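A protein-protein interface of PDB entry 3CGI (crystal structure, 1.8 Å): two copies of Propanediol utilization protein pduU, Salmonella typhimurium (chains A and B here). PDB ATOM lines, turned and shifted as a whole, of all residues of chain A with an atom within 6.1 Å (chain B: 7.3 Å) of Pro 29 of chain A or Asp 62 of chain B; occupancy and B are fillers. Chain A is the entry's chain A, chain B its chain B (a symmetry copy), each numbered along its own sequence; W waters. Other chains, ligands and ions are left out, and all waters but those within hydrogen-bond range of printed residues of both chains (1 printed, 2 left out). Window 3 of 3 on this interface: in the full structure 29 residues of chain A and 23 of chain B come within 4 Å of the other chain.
The side-chain amino group (NZ) of Lys 66 of chain B is in hydrogen-bond range of the backbone carbonyl oxygen (O) of Asn 28 of chain A (3.0 Å).
NE2 of His 24 of chain A sits at hydrogen-bond distance from OG1 of Thr 116 of chain A, at 2.9 Å. The backbone NH (N) of Ile 46 of chain A sits at hydrogen-bond distance from the backbone carbonyl oxygen (O) of Ile 26 of chain A (2.9 Å). N of Ala 27 of chain A sits at hydrogen-bond distance from O of Thr 116 of chain A. The backbone carbonyl oxygen (O) of Asp 62 of chain B sits at hydrogen-bond distance from the side-chain hydroxyl (OG1) of Thr 65 of chain B (3.4 Å). The side-chain amino group (NZ) of Lys 66 of chain B lies within salt-bridge range of the side-chain carboxylate (OD1) of Asp 62 of chain B (3.0 Å).
His 24 of chain A touches Ile 59 of chain B (CG to CD1, 3.5 Å). Asp 62 of chain B touches Ile 26 of chain A. Lys 66 of chain B touches Ile 26 of chain A (NZ to CG2, 3.9 Å). Pro 29 of chain A touches Asp 62 of chain B. O of Ile 58 of chain B touches CD2 of Leu 33 of chain A (3.5 Å). Asp 62 of chain B touches Leu 33 of chain A. Leu 75 of chain B touches Leu 33 of chain A. CG2 of Thr 116 of chain A touches OD2 of Asp 62 of chain B (3.0 Å). NZ of Lys 66 of chain B touches CG2 of Thr 116 of chain A, at 3.9 Å.
Printed residues of chain B within 4 Å of Pro 29 of chain A: Asp 62 (3.9 Å). Of chain A, only Ile 26, Pro 29, Leu 33 and Thr 116 come within 4 Å of Asp 62 of chain B. Printed residues of chain A within 4 Å of Ile 58 of chain B: Leu 33 (3.5 Å). Of the printed residues of chain A, Ile 59 of chain B touches His 24 (3.5 Å). Printed residues of chain B within 4 Å of Leu 33 of chain A: Ile 58 (3.5 Å), Asp 62 (3.9 Å) and Leu 75 (3.6 Å). Ile 46 of chain A touches none of the printed residues of chain B. The nearest residue of chain B that does not touch Pro 29 of chain A is Lys 66 of chain B (4.6 Å). The nearest residue of chain A that does not touch Asp 62 of chain B is Asn 28 of chain A (4.1 Å). The nearest printed residue of chain B that does not touch Ile 26 of chain A is Ile 58 of chain B (4.2 Å).
Of the 14 printed residues of chain A, 6 touch a printed residue of chain B. Hydrophobic or aromatic side chains of chain A within 4 Å of the printed part of chain B: His 24, Ile 26 and Leu 33. Of the 16 printed residues of chain B, 5 touch a printed residue of chain A. Hydrophobic or aromatic side chains of chain B within 4 Å of the printed part of chain A: Ile 59 and Leu 75. Among the printed residues, 10 pairs touch across the chains. Among the printed residues, no Asp or Glu carboxylate lies within 4 Å of a Lys or Arg side-chain nitrogen of the other chain.
No position is printed for both chains. Of the 10 pairs that touch across the chains among the printed residues, none has its exchanged pair printed and touching as well.
Water W1 bridges the side-chain hydroxyl (OG1) of Thr 116 of chain A (2.5 Å) and the side-chain carboxylate (OD2) of Asp 62 of chain B (2.6 Å).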
ATOM      1  N   HIS A  24      25.023  11.474  25.944  1.00  0.00           N
ATOM      2  CA  HIS A  24      24.108  10.680  25.158  1.00  0.00           C
ATOM      3  C   HIS A  24      24.654   9.331  24.845  1.00  0.00           C
ATOM      4  O   HIS A  24      25.800   9.215  24.443  1.00  0.00           O
ATOM      5  CB  HIS A  24      23.811  11.400  23.838  1.00  0.00           C
ATOM      6  CG  HIS A  24      22.768  10.718  23.025  1.00  0.00           C
ATOM      7  ND1 HIS A  24      21.430  10.986  23.171  1.00  0.00           N
ATOM      8  CD2 HIS A  24      22.863   9.751  22.080  1.00  0.00           C
ATOM      9  CE1 HIS A  24      20.736  10.204  22.367  1.00  0.00           C
ATOM     10  NE2 HIS A  24      21.585   9.458  21.679  1.00  0.00           N
ATOM     11  N   ILE A  26      24.491   5.761  22.660  1.00  0.00           N
ATOM     12  CA  ILE A  26      24.070   5.033  21.484  1.00  0.00           C
ATOM     13  C   ILE A  26      24.537   3.596  21.695  1.00  0.00           C
ATOM     14  O   ILE A  26      25.740   3.304  21.673  1.00  0.00           O
ATOM     15  CB  ILE A  26      24.627   5.632  20.154  1.00  0.00           C
ATOM     16  CG1 ILE A  26      24.265   7.125  20.065  1.00  0.00           C
ATOM     17  CG2 ILE A  26      24.047   4.892  18.950  1.00  0.00           C
ATOM     18  CD1 ILE A  26      24.681   7.852  18.800  1.00  0.00           C
ATOM     19  N   ALA A  27      23.581   2.697  21.896  1.00  0.00           N
ATOM     20  CA  ALA A  27      23.882   1.298  22.220  1.00  0.00           C
ATOM     21  C   ALA A  27      24.511   0.548  21.045  1.00  0.00           C
ATOM     22  O   ALA A  27      25.471  -0.232  21.213  1.00  0.00           O
ATOM     23  CB  ALA A  27      22.618   0.604  22.713  1.00  0.00           C
ATOM     24  N   ASN A  28      23.979   0.791  19.844  1.00  0.00           N
ATOM     25  CA  ASN A  28      24.434   0.078  18.667  1.00  0.00           C
ATOM     26  C   ASN A  28      24.681   1.033  17.510  1.00  0.00           C
ATOM     27  O   ASN A  28      23.873   1.111  16.583  1.00  0.00           O
ATOM     28  CB  ASN A  28      23.364  -0.952  18.267  1.00  0.00           C
ATOM     29  CG  ASN A  28      23.098  -1.986  19.359  1.00  0.00           C
ATOM     30  OD1 ASN A  28      22.043  -1.958  20.006  1.00  0.00           O
ATOM     31  ND2 ASN A  28      24.051  -2.892  19.576  1.00  0.00           N
ATOM     32  N   PRO A  29      25.797   1.784  17.551  1.00  0.00           N
ATOM     33  CA  PRO A  29      26.037   2.681  16.425  1.00  0.00           C
ATOM     34  C   PRO A  29      26.498   1.913  15.189  1.00  0.00           C
ATOM     35  O   PRO A  29      27.104   0.841  15.323  1.00  0.00           O
ATOM     36  CB  PRO A  29      27.153   3.590  16.931  1.00  0.00           C
ATOM     37  CG  PRO A  29      27.893   2.790  17.971  1.00  0.00           C
ATOM     38  CD  PRO A  29      26.882   1.830  18.555  1.00  0.00           C
ATOM     39  N   GLY A  30      26.234   2.457  13.999  1.00  0.00           N
ATOM     40  CA  GLY A  30      26.675   1.785  12.774  1.00  0.00           C
ATOM     41  C   GLY A  30      28.172   1.737  12.677  1.00  0.00           C
ATOM     42  O   GLY A  30      28.865   2.579  13.247  1.00  0.00           O
ATOM     43  N   LYS A  31      28.680   0.745  11.951  1.00  0.00           N
ATOM     44  CA  LYS A  31      30.111   0.597  11.723  1.00  0.00           C
ATOM     45  C   LYS A  31      30.669   1.791  10.948  1.00  0.00           C
ATOM     46  O   LYS A  31      31.775   2.255  11.225  1.00  0.00           O
ATOM     47  CB  LYS A  31      30.345  -0.723  10.987  1.00  0.00           C
ATOM     48  CG  LYS A  31      31.735  -1.012  10.478  1.00  0.00           C
ATOM     49  CD  LYS A  31      31.764  -2.454   9.984  1.00  0.00           C
ATOM     50  CE  LYS A  31      33.045  -2.804   9.245  1.00  0.00           C
ATOM     51  NZ  LYS A  31      33.094  -4.245   8.810  1.00  0.00           N
ATOM     52  N   LEU A  33      29.507   4.919  11.021  1.00  0.00           N
ATOM     53  CA  LEU A  33      29.580   6.059  11.951  1.00  0.00           C
ATOM     54  C   LEU A  33      30.794   5.894  12.869  1.00  0.00           C
ATOM     55  O   LEU A  33      31.587   6.814  13.044  1.00  0.00           O
ATOM     56  CB  LEU A  33      28.271   6.195  12.759  1.00  0.00           C
ATOM     57  CG  LEU A  33      28.155   7.244  13.876  1.00  0.00           C
ATOM     58  CD1 LEU A  33      28.566   8.634  13.403  1.00  0.00           C
ATOM     59  CD2 LEU A  33      26.752   7.293  14.430  1.00  0.00           C
ATOM     60  N   PHE A  34      30.954   4.691  13.397  1.00  0.00           N
ATOM     61  CA  PHE A  34      32.041   4.350  14.304  1.00  0.00           C
ATOM     62  C   PHE A  34      33.398   4.625  13.640  1.00  0.00           C
ATOM     63  O   PHE A  34      34.265   5.262  14.238  1.00  0.00           O
ATOM     64  CB  PHE A  34      31.897   2.873  14.700  1.00  0.00           C
ATOM     65  CG  PHE A  34      32.585   2.501  15.976  1.00  0.00           C
ATOM     66  CD1 PHE A  34      31.978   2.735  17.194  1.00  0.00           C
ATOM     67  CD2 PHE A  34      33.796   1.837  15.951  1.00  0.00           C
ATOM     68  CE1 PHE A  34      32.603   2.381  18.368  1.00  0.00           C
ATOM     69  CE2 PHE A  34      34.415   1.468  17.122  1.00  0.00           C
ATOM     70  CZ  PHE A  34      33.823   1.746  18.328  1.00  0.00           C
ATOM     71  N   VAL A  43      33.194  -2.590  16.995  1.00  0.00           N
ATOM     72  CA  VAL A  43      32.146  -1.613  17.255  1.00  0.00           C
ATOM     73  C   VAL A  43      31.544  -1.906  18.620  1.00  0.00           C
ATOM     74  O   VAL A  43      31.433  -3.077  19.012  1.00  0.00           O
ATOM     75  CB  VAL A  43      31.053  -1.634  16.177  1.00  0.00           C
ATOM     76  CG1 VAL A  43      29.870  -0.728  16.574  1.00  0.00           C
ATOM     77  CG2 VAL A  43      31.639  -1.195  14.855  1.00  0.00           C
ATOM     78  N   SER A  44      31.178  -0.857  19.350  1.00  0.00           N
ATOM     79  CA  SER A  44      30.588  -1.019  20.690  1.00  0.00           C
ATOM     80  C   SER A  44      29.636   0.119  20.929  1.00  0.00           C
ATOM     81  O   SER A  44      29.556   1.026  20.106  1.00  0.00           O
ATOM     82  CB  SER A  44      31.662  -1.010  21.785  1.00  0.00           C
ATOM     83  OG  SER A  44      32.226   0.283  22.002  1.00  0.00           O
ATOM     84  N   ALA A  45      28.954   0.116  22.070  1.00  0.00           N
ATOM     85  CA  ALA A  45      28.147   1.253  22.430  1.00  0.00           C
ATOM     86  C   ALA A  45      29.078   2.440  22.655  1.00  0.00           C
ATOM     87  O   ALA A  45      30.223   2.256  23.097  1.00  0.00           O
ATOM     88  CB  ALA A  45      27.381   0.986  23.696  1.00  0.00           C
ATOM     89  N   ILE A  46      28.562   3.638  22.402  1.00  0.00           N
ATOM     90  CA  ILE A  46      29.289   4.877  22.638  1.00  0.00           C
ATOM     91  C   ILE A  46      28.527   5.855  23.534  1.00  0.00           C
ATOM     92  O   ILE A  46      27.290   5.868  23.575  1.00  0.00           O
ATOM     93  CB  ILE A  46      29.712   5.564  21.338  1.00  0.00           C
ATOM     94  CG1 ILE A  46      28.527   5.898  20.438  1.00  0.00           C
ATOM     95  CG2 ILE A  46      30.701   4.651  20.574  1.00  0.00           C
ATOM     96  CD1 ILE A  46      28.899   6.749  19.213  1.00  0.00           C
ATOM     97  N   THR A 116      19.842   6.404  22.665  1.00  0.00           N
ATOM     98  CA  THR A 116      19.365   5.796  21.438  1.00  0.00           C
ATOM     99  C   THR A 116      19.642   4.277  21.573  1.00  0.00           C
ATOM    100  O   THR A 116      20.772   3.821  21.365  1.00  0.00           O
ATOM    101  CB  THR A 116      20.075   6.378  20.183  1.00  0.00           C
ATOM    102  OG1 THR A 116      19.818   7.784  20.070  1.00  0.00           O
ATOM    103  CG2 THR A 116      19.580   5.678  18.920  1.00  0.00           C
ATOM    104  N   ALA B  56      26.271  16.736  18.525  1.00  0.00           N
ATOM    105  CA  ALA B  56      24.962  16.171  18.192  1.00  0.00           C
ATOM    106  C   ALA B  56      24.843  15.719  16.726  1.00  0.00           C
ATOM    107  O   ALA B  56      23.939  14.990  16.385  1.00  0.00           O
ATOM    108  CB  ALA B  56      23.823  17.147  18.592  1.00  0.00           C
ATOM    109  N   SER B  57      25.753  16.156  15.854  1.00  0.00           N
ATOM    110  CA  SER B  57      25.869  15.585  14.521  1.00  0.00           C
ATOM    111  C   SER B  57      25.998  14.056  14.563  1.00  0.00           C
ATOM    112  O   SER B  57      25.548  13.375  13.649  1.00  0.00           O
ATOM    113  CB  SER B  57      27.079  16.161  13.795  1.00  0.00           C
ATOM    114  OG  SER B  57      28.275  15.901  14.515  1.00  0.00           O
ATOM    115  N   ILE B  58      26.621  13.521  15.612  1.00  0.00           N
ATOM    116  CA  ILE B  58      26.804  12.063  15.757  1.00  0.00           C
ATOM    117  C   ILE B  58      25.464  11.355  15.948  1.00  0.00           C
ATOM    118  O   ILE B  58      25.187  10.334  15.366  1.00  0.00           O
ATOM    119  CB  ILE B  58      27.775  11.745  16.926  1.00  0.00           C
ATOM    120  CG1 ILE B  58      29.174  12.333  16.599  1.00  0.00           C
ATOM    121  CG2 ILE B  58      27.790  10.244  17.218  1.00  0.00           C
ATOM    122  CD1 ILE B  58      30.167  12.358  17.765  1.00  0.00           C
ATOM    123  N   ILE B  59      24.588  11.998  16.711  1.00  0.00           N
ATOM    124  CA  ILE B  59      23.299  11.469  17.017  1.00  0.00           C
ATOM    125  C   ILE B  59      22.395  11.548  15.785  1.00  0.00           C
ATOM    126  O   ILE B  59      21.643  10.603  15.470  1.00  0.00           O
ATOM    127  CB  ILE B  59      22.663  12.309  18.166  1.00  0.00           C
ATOM    128  CG1 ILE B  59      23.624  12.438  19.371  1.00  0.00           C
ATOM    129  CG2 ILE B  59      21.340  11.679  18.585  1.00  0.00           C
ATOM    130  CD1 ILE B  59      23.003  13.243  20.578  1.00  0.00           C
ATOM    131  N   ALA B  60      22.442  12.693  15.107  1.00  0.00           N
ATOM    132  CA  ALA B  60      21.676  12.901  13.889  1.00  0.00           C
ATOM    133  C   ALA B  60      22.052  11.872  12.857  1.00  0.00           C
ATOM    134  O   ALA B  60      21.182  11.364  12.148  1.00  0.00           O
ATOM    135  CB  ALA B  60      21.896  14.313  13.336  1.00  0.00           C
ATOM    136  N   CYS B  61      23.333  11.541  12.777  1.00  0.00           N
ATOM    137  CA  CYS B  61      23.778  10.517  11.838  1.00  0.00           C
ATOM    138  C   CYS B  61      23.172   9.168  12.178  1.00  0.00           C
ATOM    139  O   CYS B  61      22.758   8.425  11.296  1.00  0.00           O
ATOM    140  CB  CYS B  61      25.290  10.370  11.834  1.00  0.00           C
ATOM    141  SG  CYS B  61      26.179  11.597  10.846  1.00  0.00           S
ATOM    142  N   ASP B  62      23.195   8.831  13.460  1.00  0.00           N
ATOM    143  CA  ASP B  62      22.643   7.560  13.903  1.00  0.00           C
ATOM    144  C   ASP B  62      21.137   7.460  13.616  1.00  0.00           C
ATOM    145  O   ASP B  62      20.671   6.462  13.066  1.00  0.00           O
ATOM    146  CB  ASP B  62      22.931   7.369  15.384  1.00  0.00           C
ATOM    147  CG  ASP B  62      22.447   6.031  15.900  1.00  0.00           C
ATOM    148  OD1 ASP B  62      23.018   4.990  15.498  1.00  0.00           O
ATOM    149  OD2 ASP B  62      21.511   6.041  16.709  1.00  0.00           O
ATOM    150  N   ILE B  63      20.378   8.486  13.993  1.00  0.00           N
ATOM    151  CA  ILE B  63      18.946   8.516  13.698  1.00  0.00           C
ATOM    152  C   ILE B  63      18.673   8.383  12.191  1.00  0.00           C
ATOM    153  O   ILE B  63      17.776   7.642  11.785  1.00  0.00           O
ATOM    154  CB  ILE B  63      18.285   9.804  14.216  1.00  0.00           C
ATOM    155  CG1 ILE B  63      18.382   9.884  15.740  1.00  0.00           C
ATOM    156  CG2 ILE B  63      16.801   9.877  13.749  1.00  0.00           C
ATOM    157  CD1 ILE B  63      18.153  11.265  16.307  1.00  0.00           C
ATOM    158  N   ALA B  64      19.476   9.060  11.366  1.00  0.00           N
ATOM    159  CA  ALA B  64      19.299   9.043   9.919  1.00  0.00           C
ATOM    160  C   ALA B  64      19.534   7.664   9.288  1.00  0.00           C
ATOM    161  O   ALA B  64      18.682   7.176   8.526  1.00  0.00           O
ATOM    162  CB  ALA B  64      20.203  10.082   9.256  1.00  0.00           C
ATOM    163  N   THR B  65      20.675   7.053   9.598  1.00  0.00           N
ATOM    164  CA  THR B  65      21.038   5.766   8.991  1.00  0.00           C
ATOM    165  C   THR B  65      20.142   4.624   9.497  1.00  0.00           C
ATOM    166  O   THR B  65      19.886   3.635   8.783  1.00  0.00           O
ATOM    167  CB  THR B  65      22.519   5.419   9.218  1.00  0.00           C
ATOM    168  OG1 THR B  65      22.799   5.348  10.629  1.00  0.00           O
ATOM    169  CG2 THR B  65      23.412   6.448   8.560  1.00  0.00           C
ATOM    170  N   LYS B  66      19.628   4.774  10.711  1.00  0.00           N
ATOM    171  CA  LYS B  66      18.701   3.788  11.249  1.00  0.00           C
ATOM    172  C   LYS B  66      17.290   3.964  10.679  1.00  0.00           C
ATOM    173  O   LYS B  66      16.514   3.020  10.696  1.00  0.00           O
ATOM    174  CB  LYS B  66      18.694   3.813  12.785  1.00  0.00           C
ATOM    175  CG  LYS B  66      19.921   3.133  13.377  1.00  0.00           C
ATOM    176  CD  LYS B  66      19.915   3.135  14.888  1.00  0.00           C
ATOM    177  CE  LYS B  66      21.189   2.476  15.455  1.00  0.00           C
ATOM    178  NZ  LYS B  66      21.420   2.867  16.879  1.00  0.00           N
ATOM    179  N   SER B  67      16.974   5.138  10.125  1.00  0.00           N
ATOM    180  CA  SER B  67      15.613   5.411   9.633  1.00  0.00           C
ATOM    181  C   SER B  67      15.280   4.761   8.301  1.00  0.00           C
ATOM    182  O   SER B  67      14.109   4.670   7.946  1.00  0.00           O
ATOM    183  CB  SER B  67      15.338   6.912   9.524  1.00  0.00           C
ATOM    184  OG  SER B  67      15.919   7.449   8.348  1.00  0.00           O
ATOM    185  N   ILE B  72      25.844   8.245   5.351  1.00  0.00           N
ATOM    186  CA  ILE B  72      26.536   9.474   5.761  1.00  0.00           C
ATOM    187  C   ILE B  72      27.475   9.856   4.612  1.00  0.00           C
ATOM    188  O   ILE B  72      28.416   9.099   4.299  1.00  0.00           O
ATOM    189  CB  ILE B  72      27.357   9.274   7.066  1.00  0.00           C
ATOM    190  CG1 ILE B  72      26.441   8.845   8.240  1.00  0.00           C
ATOM    191  CG2 ILE B  72      28.144  10.569   7.411  1.00  0.00           C
ATOM    192  CD1 ILE B  72      27.210   8.226   9.448  1.00  0.00           C
ATOM    193  N   LEU B  75      30.216  13.678   8.009  1.00  0.00           N
ATOM    194  CA  LEU B  75      29.902  14.169   9.319  1.00  0.00           C
ATOM    195  C   LEU B  75      31.000  15.157   9.726  1.00  0.00           C
ATOM    196  O   LEU B  75      32.165  14.895   9.507  1.00  0.00           O
ATOM    197  CB  LEU B  75      29.873  12.973  10.300  1.00  0.00           C
ATOM    198  CG  LEU B  75      29.876  13.193  11.800  1.00  0.00           C
ATOM    199  CD1 LEU B  75      28.780  14.140  12.158  1.00  0.00           C
ATOM    200  CD2 LEU B  75      29.709  11.885  12.517  1.00  0.00           C
ATOM    201  N   LEU B  84      23.735  13.945   4.277  1.00  0.00           N
ATOM    202  CA  LEU B  84      23.196  12.617   4.075  1.00  0.00           C
ATOM    203  C   LEU B  84      23.022  12.353   2.565  1.00  0.00           C
ATOM    204  O   LEU B  84      22.847  13.298   1.777  1.00  0.00           O
ATOM    205  CB  LEU B  84      21.838  12.541   4.751  1.00  0.00           C
ATOM    206  CG  LEU B  84      21.815  12.768   6.258  1.00  0.00           C
ATOM    207  CD1 LEU B  84      20.363  12.973   6.774  1.00  0.00           C
ATOM    208  CD2 LEU B  84      22.531  11.631   6.972  1.00  0.00           C
ATOM    209  N   VAL B  98      15.292  12.974  12.217  1.00  0.00           N
ATOM    210  CA  VAL B  98      16.319  13.705  12.979  1.00  0.00           C
ATOM    211  C   VAL B  98      15.628  14.848  13.735  1.00  0.00           C
ATOM    212  O   VAL B  98      15.763  14.976  14.949  1.00  0.00           O
ATOM    213  CB  VAL B  98      17.402  14.228  12.087  1.00  0.00           C
ATOM    214  CG1 VAL B  98      18.263  15.275  12.856  1.00  0.00           C
ATOM    215  CG2 VAL B  98      18.303  13.043  11.554  1.00  0.00           C
HETATM  216  O   HOH W   1      21.255   8.277  18.081  1.00  0.00           O
